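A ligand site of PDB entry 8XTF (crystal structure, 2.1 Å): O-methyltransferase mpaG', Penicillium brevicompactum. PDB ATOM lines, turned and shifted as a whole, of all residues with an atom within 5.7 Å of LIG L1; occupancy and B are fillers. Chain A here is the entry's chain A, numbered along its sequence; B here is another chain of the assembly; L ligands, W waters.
Water W3 lies within hydrogen-bond range of O5 of LIG L1 (2.8 Å), O of Pro 185 (3.4 Å) and N of Gln 186 (3.4 Å). Water W1 lies within hydrogen-bond range of OH of Tyr 201, OG of Ser 146 and O4 of LIG L1. Water W2 lies within hydrogen-bond range of OD1 of Asn 199 (2.7 Å), O5 of LG2 L2 (2.8 Å) and NE2 of Gln 269 (2.9 Å).
Merely in contact with LIG L1: Phe 184 (3.6 Å), Pro 185 (3.7 Å), Leu 188 (3.8 Å), Val 189 (3.8 Å), Phe 198 (3.6 Å), Met 202 (3.6 Å), Tyr 205 (3.6 Å), Val 306 (3.6 Å), Phe 310 (3.99 Å), Ile 355 (3.5 Å), Met 356 (3.4 Å), Met 360 (3.9 Å) and Trp 56 of chain B (3.8 Å). Hydrophobic or aromatic side chains within 4 Å of LIG L1: Phe 184, Pro 185, Leu 188, Val 189, Phe 198, Tyr 201, Met 202, Tyr 205, His 308, Phe 310, Ile 355, Met 356, His 359, Met 360 and Trp 56 of chain B. Of the 26 residues printed, 19 come within 4 Å of LIG L1. The nearest printed residue that does not touch LIG L1 is Phe 141 (4.1 Å).
The side-chain hydroxyl (OG) of Ser 146 lies within hydrogen-bond range of a ring nitrogen (NE2) of His 359, at 2.8 Å. NE1 of Trp 56 of chain B sits at hydrogen-bond distance from OH of Tyr 201 (2.6 Å). OH of Tyr 205 is in hydrogen-bond range of OG of Ser 305 (2.8 Å). ND1 of His 359 is in hydrogen-bond range of O of Ile 355, at 2.9 Å. ND1 of His 308 lies close to SD of Met 356, at 3.6 Å. A ring nitrogen (NE2) of His 308 sits at hydrogen-bond distance from the backbone carbonyl oxygen of Ser 305. ND2 of Asn 199 is in hydrogen-bond range of OE1 of Gln 269, at 3.0 Å.
An oxygen (O2) of LIG L1 sits close to a sulfur (S1) of LG2 L2, 3.5 Å away.
An oxygen (O2) of LG2 L2 lies within hydrogen-bond range of the side-chain hydroxyl of Tyr 205, at 2.7 Å. O4 of LIG L1 lies close to NE2 of His 359, at 3.5 Å. The side-chain hydroxyl (OH) of Tyr 201 sits close to an oxygen (O3) of LIG L1 (3.3 Å). The backbone carbonyl oxygen (O) of Ser 305 lies within hydrogen-bond range of an oxygen (O2) of LIG L1 (3.2 Å). The side-chain amide nitrogen (NE2) of Gln 269 sits at hydrogen-bond distance from an oxygen (O6) of LIG L1, 2.8 Å away. NH2 of Arg 267 is in salt-bridge range of O5 of LIG L1, 2.9 Å away. A ring nitrogen (NE2) of His 308 lies within hydrogen-bond range of an oxygen (O2) of LIG L1, at 2.9 Å.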
ATOM      1  N   PHE A 141      -1.499  19.309  11.059  1.00  0.00           N
ATOM      2  CA  PHE A 141      -1.748  19.709   9.684  1.00  0.00           C
ATOM      3  C   PHE A 141      -1.943  18.486   8.781  1.00  0.00           C
ATOM      4  O   PHE A 141      -2.929  18.401   8.055  1.00  0.00           O
ATOM      5  CB  PHE A 141      -0.588  20.561   9.142  1.00  0.00           C
ATOM      6  CG  PHE A 141      -0.882  21.175   7.804  1.00  0.00           C
ATOM      7  CD1 PHE A 141      -0.645  20.463   6.639  1.00  0.00           C
ATOM      8  CD2 PHE A 141      -1.455  22.427   7.724  1.00  0.00           C
ATOM      9  CE1 PHE A 141      -0.949  21.002   5.412  1.00  0.00           C
ATOM     10  CE2 PHE A 141      -1.752  22.977   6.492  1.00  0.00           C
ATOM     11  CZ  PHE A 141      -1.511  22.274   5.332  1.00  0.00           C
ATOM     12  N   SER A 146      -4.055  17.299   5.050  1.00  0.00           N
ATOM     13  CA  SER A 146      -3.501  16.526   3.948  1.00  0.00           C
ATOM     14  C   SER A 146      -4.182  15.166   3.798  1.00  0.00           C
ATOM     15  O   SER A 146      -4.533  14.760   2.685  1.00  0.00           O
ATOM     16  CB  SER A 146      -1.991  16.325   4.133  1.00  0.00           C
ATOM     17  OG  SER A 146      -1.376  17.552   4.468  1.00  0.00           O
ATOM     18  N   PHE A 184      -6.029  26.231  -2.199  1.00  0.00           N
ATOM     19  CA  PHE A 184      -5.401  25.875  -0.935  1.00  0.00           C
ATOM     20  C   PHE A 184      -4.829  27.070  -0.173  1.00  0.00           C
ATOM     21  O   PHE A 184      -5.091  27.167   1.039  1.00  0.00           O
ATOM     22  CB  PHE A 184      -4.324  24.816  -1.222  1.00  0.00           C
ATOM     23  CG  PHE A 184      -3.411  24.499  -0.062  1.00  0.00           C
ATOM     24  CD1 PHE A 184      -3.871  23.734   1.007  1.00  0.00           C
ATOM     25  CD2 PHE A 184      -2.072  24.894  -0.076  1.00  0.00           C
ATOM     26  CE1 PHE A 184      -3.022  23.416   2.064  1.00  0.00           C
ATOM     27  CE2 PHE A 184      -1.221  24.559   0.964  1.00  0.00           C
ATOM     28  CZ  PHE A 184      -1.694  23.811   2.036  1.00  0.00           C
ATOM     29  N   PRO A 185      -4.081  27.999  -0.784  1.00  0.00           N
ATOM     30  CA  PRO A 185      -3.631  29.179  -0.012  1.00  0.00           C
ATOM     31  C   PRO A 185      -4.777  30.000   0.551  1.00  0.00           C
ATOM     32  O   PRO A 185      -4.691  30.465   1.700  1.00  0.00           O
ATOM     33  CB  PRO A 185      -2.787  29.985  -1.018  1.00  0.00           C
ATOM     34  CG  PRO A 185      -2.326  28.962  -2.017  1.00  0.00           C
ATOM     35  CD  PRO A 185      -3.485  27.984  -2.137  1.00  0.00           C
ATOM     36  N   GLN A 186      -5.839  30.213  -0.223  1.00  0.00           N
ATOM     37  CA  GLN A 186      -6.998  30.921   0.283  1.00  0.00           C
ATOM     38  C   GLN A 186      -7.705  30.144   1.387  1.00  0.00           C
ATOM     39  O   GLN A 186      -8.249  30.735   2.324  1.00  0.00           O
ATOM     40  CB  GLN A 186      -7.980  31.221  -0.845  1.00  0.00           C
ATOM     41  CG  GLN A 186      -7.503  32.320  -1.784  1.00  0.00           C
ATOM     42  CD  GLN A 186      -8.273  32.368  -3.099  1.00  0.00           C
ATOM     43  OE1 GLN A 186      -9.167  31.555  -3.355  1.00  0.00           O
ATOM     44  NE2 GLN A 186      -7.904  33.315  -3.945  1.00  0.00           N
ATOM     45  N   LEU A 188      -6.213  28.223   3.568  1.00  0.00           N
ATOM     46  CA  LEU A 188      -5.439  28.347   4.807  1.00  0.00           C
ATOM     47  C   LEU A 188      -5.733  29.660   5.495  1.00  0.00           C
ATOM     48  O   LEU A 188      -5.946  29.701   6.719  1.00  0.00           O
ATOM     49  CB  LEU A 188      -3.934  28.231   4.508  1.00  0.00           C
ATOM     50  CG  LEU A 188      -3.398  26.842   4.187  1.00  0.00           C
ATOM     51  CD1 LEU A 188      -1.999  26.960   3.678  1.00  0.00           C
ATOM     52  CD2 LEU A 188      -3.473  25.938   5.427  1.00  0.00           C
ATOM     53  N   VAL A 189      -5.764  30.757   4.741  1.00  0.00           N
ATOM     54  CA  VAL A 189      -6.057  32.064   5.296  1.00  0.00           C
ATOM     55  C   VAL A 189      -7.433  32.063   5.965  1.00  0.00           C
ATOM     56  O   VAL A 189      -7.621  32.666   7.024  1.00  0.00           O
ATOM     57  CB  VAL A 189      -5.961  33.142   4.204  1.00  0.00           C
ATOM     58  CG1 VAL A 189      -6.499  34.495   4.696  1.00  0.00           C
ATOM     59  CG2 VAL A 189      -4.516  33.262   3.717  1.00  0.00           C
ATOM     60  N   LEU A 195      -3.152  27.780   9.024  1.00  0.00           N
ATOM     61  CA  LEU A 195      -2.139  28.582   8.341  1.00  0.00           C
ATOM     62  C   LEU A 195      -0.879  28.677   9.180  1.00  0.00           C
ATOM     63  O   LEU A 195       0.236  28.457   8.683  1.00  0.00           O
ATOM     64  CB  LEU A 195      -2.674  29.974   8.016  1.00  0.00           C
ATOM     65  CG  LEU A 195      -1.706  30.925   7.303  1.00  0.00           C
ATOM     66  CD1 LEU A 195      -1.053  30.306   6.064  1.00  0.00           C
ATOM     67  CD2 LEU A 195      -2.431  32.214   6.938  1.00  0.00           C
ATOM     68  N   PHE A 198       0.819  25.396   9.211  1.00  0.00           N
ATOM     69  CA  PHE A 198       1.604  25.255   7.986  1.00  0.00           C
ATOM     70  C   PHE A 198       2.973  25.907   8.120  1.00  0.00           C
ATOM     71  O   PHE A 198       3.987  25.319   7.745  1.00  0.00           O
ATOM     72  CB  PHE A 198       0.841  25.851   6.803  1.00  0.00           C
ATOM     73  CG  PHE A 198       1.522  25.639   5.484  1.00  0.00           C
ATOM     74  CD1 PHE A 198       1.308  24.456   4.767  1.00  0.00           C
ATOM     75  CD2 PHE A 198       2.368  26.605   4.944  1.00  0.00           C
ATOM     76  CE1 PHE A 198       1.934  24.253   3.537  1.00  0.00           C
ATOM     77  CE2 PHE A 198       2.994  26.402   3.713  1.00  0.00           C
ATOM     78  CZ  PHE A 198       2.771  25.225   3.018  1.00  0.00           C
ATOM     79  N   ASN A 199       3.006  27.124   8.686  1.00  0.00           N
ATOM     80  CA  ASN A 199       4.275  27.842   8.788  1.00  0.00           C
ATOM     81  C   ASN A 199       5.249  27.136   9.727  1.00  0.00           C
ATOM     82  O   ASN A 199       6.461  27.156   9.487  1.00  0.00           O
ATOM     83  CB  ASN A 199       4.026  29.287   9.241  1.00  0.00           C
ATOM     84  CG  ASN A 199       3.292  30.134   8.193  1.00  0.00           C
ATOM     85  OD1 ASN A 199       3.353  29.876   6.993  1.00  0.00           O
ATOM     86  ND2 ASN A 199       2.586  31.155   8.662  1.00  0.00           N
ATOM     87  N   TYR A 201       5.186  23.841  10.210  1.00  0.00           N
ATOM     88  CA  TYR A 201       5.463  22.678   9.388  1.00  0.00           C
ATOM     89  C   TYR A 201       6.616  22.900   8.410  1.00  0.00           C
ATOM     90  O   TYR A 201       7.391  21.981   8.160  1.00  0.00           O
ATOM     91  CB  TYR A 201       4.168  22.357   8.641  1.00  0.00           C
ATOM     92  CG  TYR A 201       4.058  21.126   7.789  1.00  0.00           C
ATOM     93  CD1 TYR A 201       4.860  20.012   7.997  1.00  0.00           C
ATOM     94  CD2 TYR A 201       3.099  21.075   6.797  1.00  0.00           C
ATOM     95  CE1 TYR A 201       4.695  18.875   7.211  1.00  0.00           C
ATOM     96  CE2 TYR A 201       2.936  19.962   6.010  1.00  0.00           C
ATOM     97  CZ  TYR A 201       3.727  18.869   6.212  1.00  0.00           C
ATOM     98  OH  TYR A 201       3.531  17.778   5.392  1.00  0.00           O
ATOM     99  N   MET A 202       6.742  24.112   7.857  1.00  0.00           N
ATOM    100  CA  MET A 202       7.813  24.328   6.879  1.00  0.00           C
ATOM    101  C   MET A 202       9.207  24.191   7.476  1.00  0.00           C
ATOM    102  O   MET A 202      10.151  23.873   6.760  1.00  0.00           O
ATOM    103  CB  MET A 202       7.662  25.693   6.209  1.00  0.00           C
ATOM    104  CG  MET A 202       6.425  25.786   5.315  1.00  0.00           C
ATOM    105  SD  MET A 202       6.296  24.455   4.092  1.00  0.00           S
ATOM    106  CE  MET A 202       5.122  23.359   4.888  1.00  0.00           C
ATOM    107  N   TYR A 205       9.370  19.757   7.659  1.00  0.00           N
ATOM    108  CA  TYR A 205       9.115  18.713   6.657  1.00  0.00           C
ATOM    109  C   TYR A 205      10.406  18.099   6.098  1.00  0.00           C
ATOM    110  O   TYR A 205      10.393  16.949   5.649  1.00  0.00           O
ATOM    111  CB  TYR A 205       8.253  19.232   5.509  1.00  0.00           C
ATOM    112  CG  TYR A 205       8.959  20.144   4.532  1.00  0.00           C
ATOM    113  CD1 TYR A 205       9.145  21.478   4.828  1.00  0.00           C
ATOM    114  CD2 TYR A 205       9.422  19.679   3.306  1.00  0.00           C
ATOM    115  CE1 TYR A 205       9.788  22.343   3.961  1.00  0.00           C
ATOM    116  CE2 TYR A 205      10.076  20.541   2.407  1.00  0.00           C
ATOM    117  CZ  TYR A 205      10.257  21.870   2.744  1.00  0.00           C
ATOM    118  OH  TYR A 205      10.915  22.764   1.902  1.00  0.00           O
ATOM    119  N   ARG A 267       5.061  36.294   2.978  1.00  0.00           N
ATOM    120  CA  ARG A 267       3.782  36.932   3.232  1.00  0.00           C
ATOM    121  C   ARG A 267       3.774  37.637   4.591  1.00  0.00           C
ATOM    122  O   ARG A 267       4.452  37.227   5.540  1.00  0.00           O
ATOM    123  CB  ARG A 267       2.646  35.914   3.169  1.00  0.00           C
ATOM    124  CG  ARG A 267       2.693  35.057   1.926  1.00  0.00           C
ATOM    125  CD  ARG A 267       2.132  35.818   0.744  1.00  0.00           C
ATOM    126  NE  ARG A 267       0.674  35.836   0.820  1.00  0.00           N
ATOM    127  CZ  ARG A 267      -0.110  36.544   0.025  1.00  0.00           C
ATOM    128  NH1 ARG A 267       0.380  37.330  -0.920  1.00  0.00           N
ATOM    129  NH2 ARG A 267      -1.434  36.437   0.162  1.00  0.00           N
ATOM    130  N   GLN A 269       1.507  37.624   6.873  1.00  0.00           N
ATOM    131  CA  GLN A 269       1.095  36.785   7.991  1.00  0.00           C
ATOM    132  C   GLN A 269       2.223  35.848   8.442  1.00  0.00           C
ATOM    133  O   GLN A 269       2.231  35.409   9.603  1.00  0.00           O
ATOM    134  CB  GLN A 269      -0.150  35.969   7.638  1.00  0.00           C
ATOM    135  CG  GLN A 269      -0.065  35.219   6.314  1.00  0.00           C
ATOM    136  CD  GLN A 269       0.591  33.849   6.445  1.00  0.00           C
ATOM    137  OE1 GLN A 269       0.886  33.370   7.561  1.00  0.00           O
ATOM    138  NE2 GLN A 269       0.831  33.208   5.308  1.00  0.00           N
ATOM    139  N   SER A 305      11.484  25.269  -2.481  1.00  0.00           N
ATOM    140  CA  SER A 305      10.106  24.757  -2.488  1.00  0.00           C
ATOM    141  C   SER A 305       9.079  25.876  -2.693  1.00  0.00           C
ATOM    142  O   SER A 305       8.122  26.005  -1.908  1.00  0.00           O
ATOM    143  CB  SER A 305       9.765  24.015  -1.195  1.00  0.00           C
ATOM    144  OG  SER A 305      10.668  22.967  -0.905  1.00  0.00           O
ATOM    145  N   VAL A 306       9.288  26.704  -3.699  1.00  0.00           N
ATOM    146  CA  VAL A 306       8.312  27.768  -3.946  1.00  0.00           C
ATOM    147  C   VAL A 306       7.662  27.570  -5.314  1.00  0.00           C
ATOM    148  O   VAL A 306       6.465  27.244  -5.338  1.00  0.00           O
ATOM    149  CB  VAL A 306       8.953  29.160  -3.771  1.00  0.00           C
ATOM    150  CG1 VAL A 306       8.026  30.275  -4.294  1.00  0.00           C
ATOM    151  CG2 VAL A 306       9.325  29.376  -2.299  1.00  0.00           C
ATOM    152  N   HIS A 308       7.639  25.083  -7.221  1.00  0.00           N
ATOM    153  CA  HIS A 308       7.124  23.734  -7.415  1.00  0.00           C
ATOM    154  C   HIS A 308       5.640  23.637  -7.082  1.00  0.00           C
ATOM    155  O   HIS A 308       4.998  22.670  -7.490  1.00  0.00           O
ATOM    156  CB  HIS A 308       7.928  22.706  -6.594  1.00  0.00           C
ATOM    157  CG  HIS A 308       7.573  22.667  -5.138  1.00  0.00           C
ATOM    158  ND1 HIS A 308       7.574  21.493  -4.398  1.00  0.00           N
ATOM    159  CD2 HIS A 308       7.229  23.645  -4.270  1.00  0.00           C
ATOM    160  CE1 HIS A 308       7.242  21.757  -3.151  1.00  0.00           C
ATOM    161  NE2 HIS A 308       7.025  23.050  -3.044  1.00  0.00           N
ATOM    162  N   GLY A 309       5.076  24.618  -6.386  1.00  0.00           N
ATOM    163  CA  GLY A 309       3.670  24.580  -6.056  1.00  0.00           C
ATOM    164  C   GLY A 309       2.777  25.286  -7.053  1.00  0.00           C
ATOM    165  O   GLY A 309       1.571  25.446  -6.809  1.00  0.00           O
ATOM    166  N   PHE A 310       3.329  25.687  -8.205  1.00  0.00           N
ATOM    167  CA  PHE A 310       2.620  26.504  -9.171  1.00  0.00           C
ATOM    168  C   PHE A 310       2.726  25.872 -10.556  1.00  0.00           C
ATOM    169  O   PHE A 310       3.730  25.247 -10.893  1.00  0.00           O
ATOM    170  CB  PHE A 310       3.190  27.942  -9.161  1.00  0.00           C
ATOM    171  CG  PHE A 310       2.948  28.653  -7.866  1.00  0.00           C
ATOM    172  CD1 PHE A 310       1.762  29.335  -7.650  1.00  0.00           C
ATOM    173  CD2 PHE A 310       3.878  28.590  -6.836  1.00  0.00           C
ATOM    174  CE1 PHE A 310       1.503  29.964  -6.444  1.00  0.00           C
ATOM    175  CE2 PHE A 310       3.636  29.231  -5.623  1.00  0.00           C
ATOM    176  CZ  PHE A 310       2.441  29.916  -5.429  1.00  0.00           C
ATOM    177  N   MET A 352       6.738  14.276  -2.525  1.00  0.00           N
ATOM    178  CA  MET A 352       6.460  15.690  -2.693  1.00  0.00           C
ATOM    179  C   MET A 352       5.584  15.928  -3.906  1.00  0.00           C
ATOM    180  O   MET A 352       4.709  16.794  -3.886  1.00  0.00           O
ATOM    181  CB  MET A 352       7.777  16.464  -2.799  1.00  0.00           C
ATOM    182  CG  MET A 352       7.644  17.977  -2.676  1.00  0.00           C
ATOM    183  SD  MET A 352       6.858  18.555  -1.166  1.00  0.00           S
ATOM    184  CE  MET A 352       8.268  18.481  -0.048  1.00  0.00           C
ATOM    185  N   ILE A 355       2.137  15.252  -2.791  1.00  0.00           N
ATOM    186  CA  ILE A 355       1.749  16.341  -1.903  1.00  0.00           C
ATOM    187  C   ILE A 355       1.374  17.576  -2.720  1.00  0.00           C
ATOM    188  O   ILE A 355       0.342  18.207  -2.464  1.00  0.00           O
ATOM    189  CB  ILE A 355       2.877  16.644  -0.896  1.00  0.00           C
ATOM    190  CG1 ILE A 355       2.930  15.589   0.218  1.00  0.00           C
ATOM    191  CG2 ILE A 355       2.707  18.035  -0.270  1.00  0.00           C
ATOM    192  CD1 ILE A 355       1.792  15.716   1.244  1.00  0.00           C
ATOM    193  N   MET A 356       2.159  17.913  -3.741  1.00  0.00           N
ATOM    194  CA  MET A 356       1.784  19.038  -4.611  1.00  0.00           C
ATOM    195  C   MET A 356       0.442  18.803  -5.281  1.00  0.00           C
ATOM    196  O   MET A 356      -0.386  19.709  -5.366  1.00  0.00           O
ATOM    197  CB  MET A 356       2.854  19.311  -5.677  1.00  0.00           C
ATOM    198  CG  MET A 356       4.155  19.824  -5.097  1.00  0.00           C
ATOM    199  SD  MET A 356       3.953  21.346  -4.133  1.00  0.00           S
ATOM    200  CE  MET A 356       3.968  20.660  -2.461  1.00  0.00           C
ATOM    201  N   HIS A 359      -2.519  19.215  -2.633  1.00  0.00           N
ATOM    202  CA  HIS A 359      -2.779  20.521  -2.038  1.00  0.00           C
ATOM    203  C   HIS A 359      -2.920  21.606  -3.096  1.00  0.00           C
ATOM    204  O   HIS A 359      -3.892  22.355  -3.088  1.00  0.00           O
ATOM    205  CB  HIS A 359      -1.670  20.893  -1.053  1.00  0.00           C
ATOM    206  CG  HIS A 359      -1.583  19.991   0.139  1.00  0.00           C
ATOM    207  ND1 HIS A 359      -0.878  18.811   0.135  1.00  0.00           N
ATOM    208  CD2 HIS A 359      -2.121  20.106   1.379  1.00  0.00           C
ATOM    209  CE1 HIS A 359      -0.994  18.227   1.321  1.00  0.00           C
ATOM    210  NE2 HIS A 359      -1.743  18.997   2.090  1.00  0.00           N
ATOM    211  N   MET A 360      -1.948  21.707  -3.987  1.00  0.00           N
ATOM    212  CA  MET A 360      -1.869  22.784  -4.963  1.00  0.00           C
ATOM    213  C   MET A 360      -2.364  22.365  -6.345  1.00  0.00           C
ATOM    214  O   MET A 360      -2.454  23.218  -7.238  1.00  0.00           O
ATOM    215  CB  MET A 360      -0.407  23.256  -5.062  1.00  0.00           C
ATOM    216  CG  MET A 360       0.092  24.130  -3.901  1.00  0.00           C
ATOM    217  SD  MET A 360      -0.960  25.556  -3.536  1.00  0.00           S
ATOM    218  CE  MET A 360      -0.044  26.865  -4.391  1.00  0.00           C
ATOM    219  N   TRP B  56       2.675  11.177   4.285  1.00  0.00           N
ATOM    220  CA  TRP B  56       2.641  11.401   2.839  1.00  0.00           C
ATOM    221  C   TRP B  56       2.658  10.095   2.055  1.00  0.00           C
ATOM    222  O   TRP B  56       1.713   9.790   1.332  1.00  0.00           O
ATOM    223  CB  TRP B  56       3.809  12.272   2.351  1.00  0.00           C
ATOM    224  CG  TRP B  56       4.014  13.585   3.038  1.00  0.00           C
ATOM    225  CD1 TRP B  56       3.297  14.113   4.084  1.00  0.00           C
ATOM    226  CD2 TRP B  56       5.034  14.530   2.728  1.00  0.00           C
ATOM    227  NE1 TRP B  56       3.822  15.343   4.433  1.00  0.00           N
ATOM    228  CE2 TRP B  56       4.886  15.621   3.608  1.00  0.00           C
ATOM    229  CE3 TRP B  56       6.065  14.570   1.773  1.00  0.00           C
ATOM    230  CZ2 TRP B  56       5.712  16.730   3.566  1.00  0.00           C
ATOM    231  CZ3 TRP B  56       6.878  15.675   1.726  1.00  0.00           C
ATOM    232  CH2 TRP B  56       6.713  16.737   2.635  1.00  0.00           C
HETATM  233  C1  LIG L   1       1.279  27.859  -0.241  1.00  0.00           C
HETATM  234  C2  LIG L   1       4.185  26.756  -2.539  1.00  0.00           C
HETATM  235  C3  LIG L   1       0.668  29.816   1.240  1.00  0.00           C
HETATM  236  C4  LIG L   1       0.880  29.133   2.555  1.00  0.00           C
HETATM  237  C5  LIG L   1      -0.866  31.704   2.048  1.00  0.00           C
HETATM  238  C6  LIG L   1       3.604  23.266  -0.315  1.00  0.00           C
HETATM  239  C7  LIG L   1       2.623  25.557  -1.009  1.00  0.00           C
HETATM  240  C8  LIG L   1       3.058  26.688  -1.551  1.00  0.00           C
HETATM  241  C9  LIG L   1       2.442  28.016  -1.197  1.00  0.00           C
HETATM  242  C10 LIG L   1       0.705  29.197   0.073  1.00  0.00           C
HETATM  243  C11 LIG L   1       7.006  22.424   1.227  1.00  0.00           C
HETATM  244  C12 LIG L   1       0.407  31.299   1.311  1.00  0.00           C
HETATM  245  C13 LIG L   1       4.976  23.258  -0.025  1.00  0.00           C
HETATM  246  C14 LIG L   1      -1.131  33.196   2.055  1.00  0.00           C
HETATM  247  C15 LIG L   1       5.524  22.395   0.930  1.00  0.00           C
HETATM  248  C16 LIG L   1       4.674  21.534   1.585  1.00  0.00           C
HETATM  249  C17 LIG L   1       3.329  21.509   1.310  1.00  0.00           C
HETATM  250  C18 LIG L   1       2.781  22.371   0.356  1.00  0.00           C
HETATM  251  C19 LIG L   1       4.949  20.508   2.632  1.00  0.00           C
HETATM  252  C20 LIG L   1       2.695  20.490   2.155  1.00  0.00           C
HETATM  253  C21 LIG L   1       3.046  24.164  -1.401  1.00  0.00           C
HETATM  254  O1  LIG L   1       1.467  22.360   0.072  1.00  0.00           O
HETATM  255  O2  LIG L   1       5.804  24.121  -0.663  1.00  0.00           O
HETATM  256  O3  LIG L   1       3.668  19.874   2.865  1.00  0.00           O
HETATM  257  O4  LIG L   1       1.549  20.165   2.296  1.00  0.00           O
HETATM  258  O5  LIG L   1      -1.784  33.672   1.094  1.00  0.00           O
HETATM  259  O6  LIG L   1      -0.677  33.889   3.005  1.00  0.00           O
HETATM  260  N1  LG2 L   2      11.033  28.227   1.737  1.00  0.00           N
HETATM  261  C1  LG2 L   2      10.400  27.591   2.901  1.00  0.00           C
HETATM  262  C2  LG2 L   2       8.873  27.575   2.772  1.00  0.00           C
HETATM  263  C3  LG2 L   2       8.367  26.809   1.553  1.00  0.00           C
HETATM  264  S1  LG2 L   2       6.557  26.695   1.517  1.00  0.00           S
HETATM  265  C4  LG2 L   2      10.877  26.148   3.116  1.00  0.00           C
HETATM  266  O1  LG2 L   2      10.949  25.659   4.262  1.00  0.00           O
HETATM  267  O2  LG2 L   2      11.187  25.438   2.144  1.00  0.00           O
HETATM  268  C5  LG2 L   2       6.254  28.019   0.324  1.00  0.00           C
HETATM  269  C6  LG2 L   2       6.418  29.434   0.876  1.00  0.00           C
HETATM  270  O3  LG2 L   2       6.028  30.377  -0.131  1.00  0.00           O
HETATM  271  C7  LG2 L   2       5.554  29.744   2.090  1.00  0.00           C
HETATM  272  O4  LG2 L   2       6.383  30.294   3.086  1.00  0.00           O
HETATM  273  C8  LG2 L   2       4.554  30.788   1.589  1.00  0.00           C
HETATM  274  O5  LG2 L   2       4.112  31.718   2.558  1.00  0.00           O
HETATM  275  C9  LG2 L   2       5.311  31.445   0.452  1.00  0.00           C
HETATM  276  N2  LG2 L   2       4.438  32.127  -0.517  1.00  0.00           N
HETATM  277  C10 LG2 L   2       3.367  31.593  -1.170  1.00  0.00           C
HETATM  278  N3  LG2 L   2       2.833  32.533  -1.972  1.00  0.00           N
HETATM  279  C11 LG2 L   2       3.535  33.677  -1.833  1.00  0.00           C
HETATM  280  C12 LG2 L   2       3.413  34.954  -2.409  1.00  0.00           C
HETATM  281  N4  LG2 L   2       2.446  35.233  -3.289  1.00  0.00           N
HETATM  282  N5  LG2 L   2       4.331  35.921  -2.067  1.00  0.00           N
HETATM  283  C13 LG2 L   2       5.319  35.642  -1.160  1.00  0.00           C
HETATM  284  N6  LG2 L   2       5.432  34.389  -0.598  1.00  0.00           N
HETATM  285  C14 LG2 L   2       4.558  33.420  -0.931  1.00  0.00           C
HETATM  286  O   HOH W   1       1.304  17.963   4.013  1.00  0.00           O
HETATM  287  O   HOH W   2       2.460  30.936   4.651  1.00  0.00           O
HETATM  288  O   HOH W   3      -4.164  33.154  -0.248  1.00  0.00           O
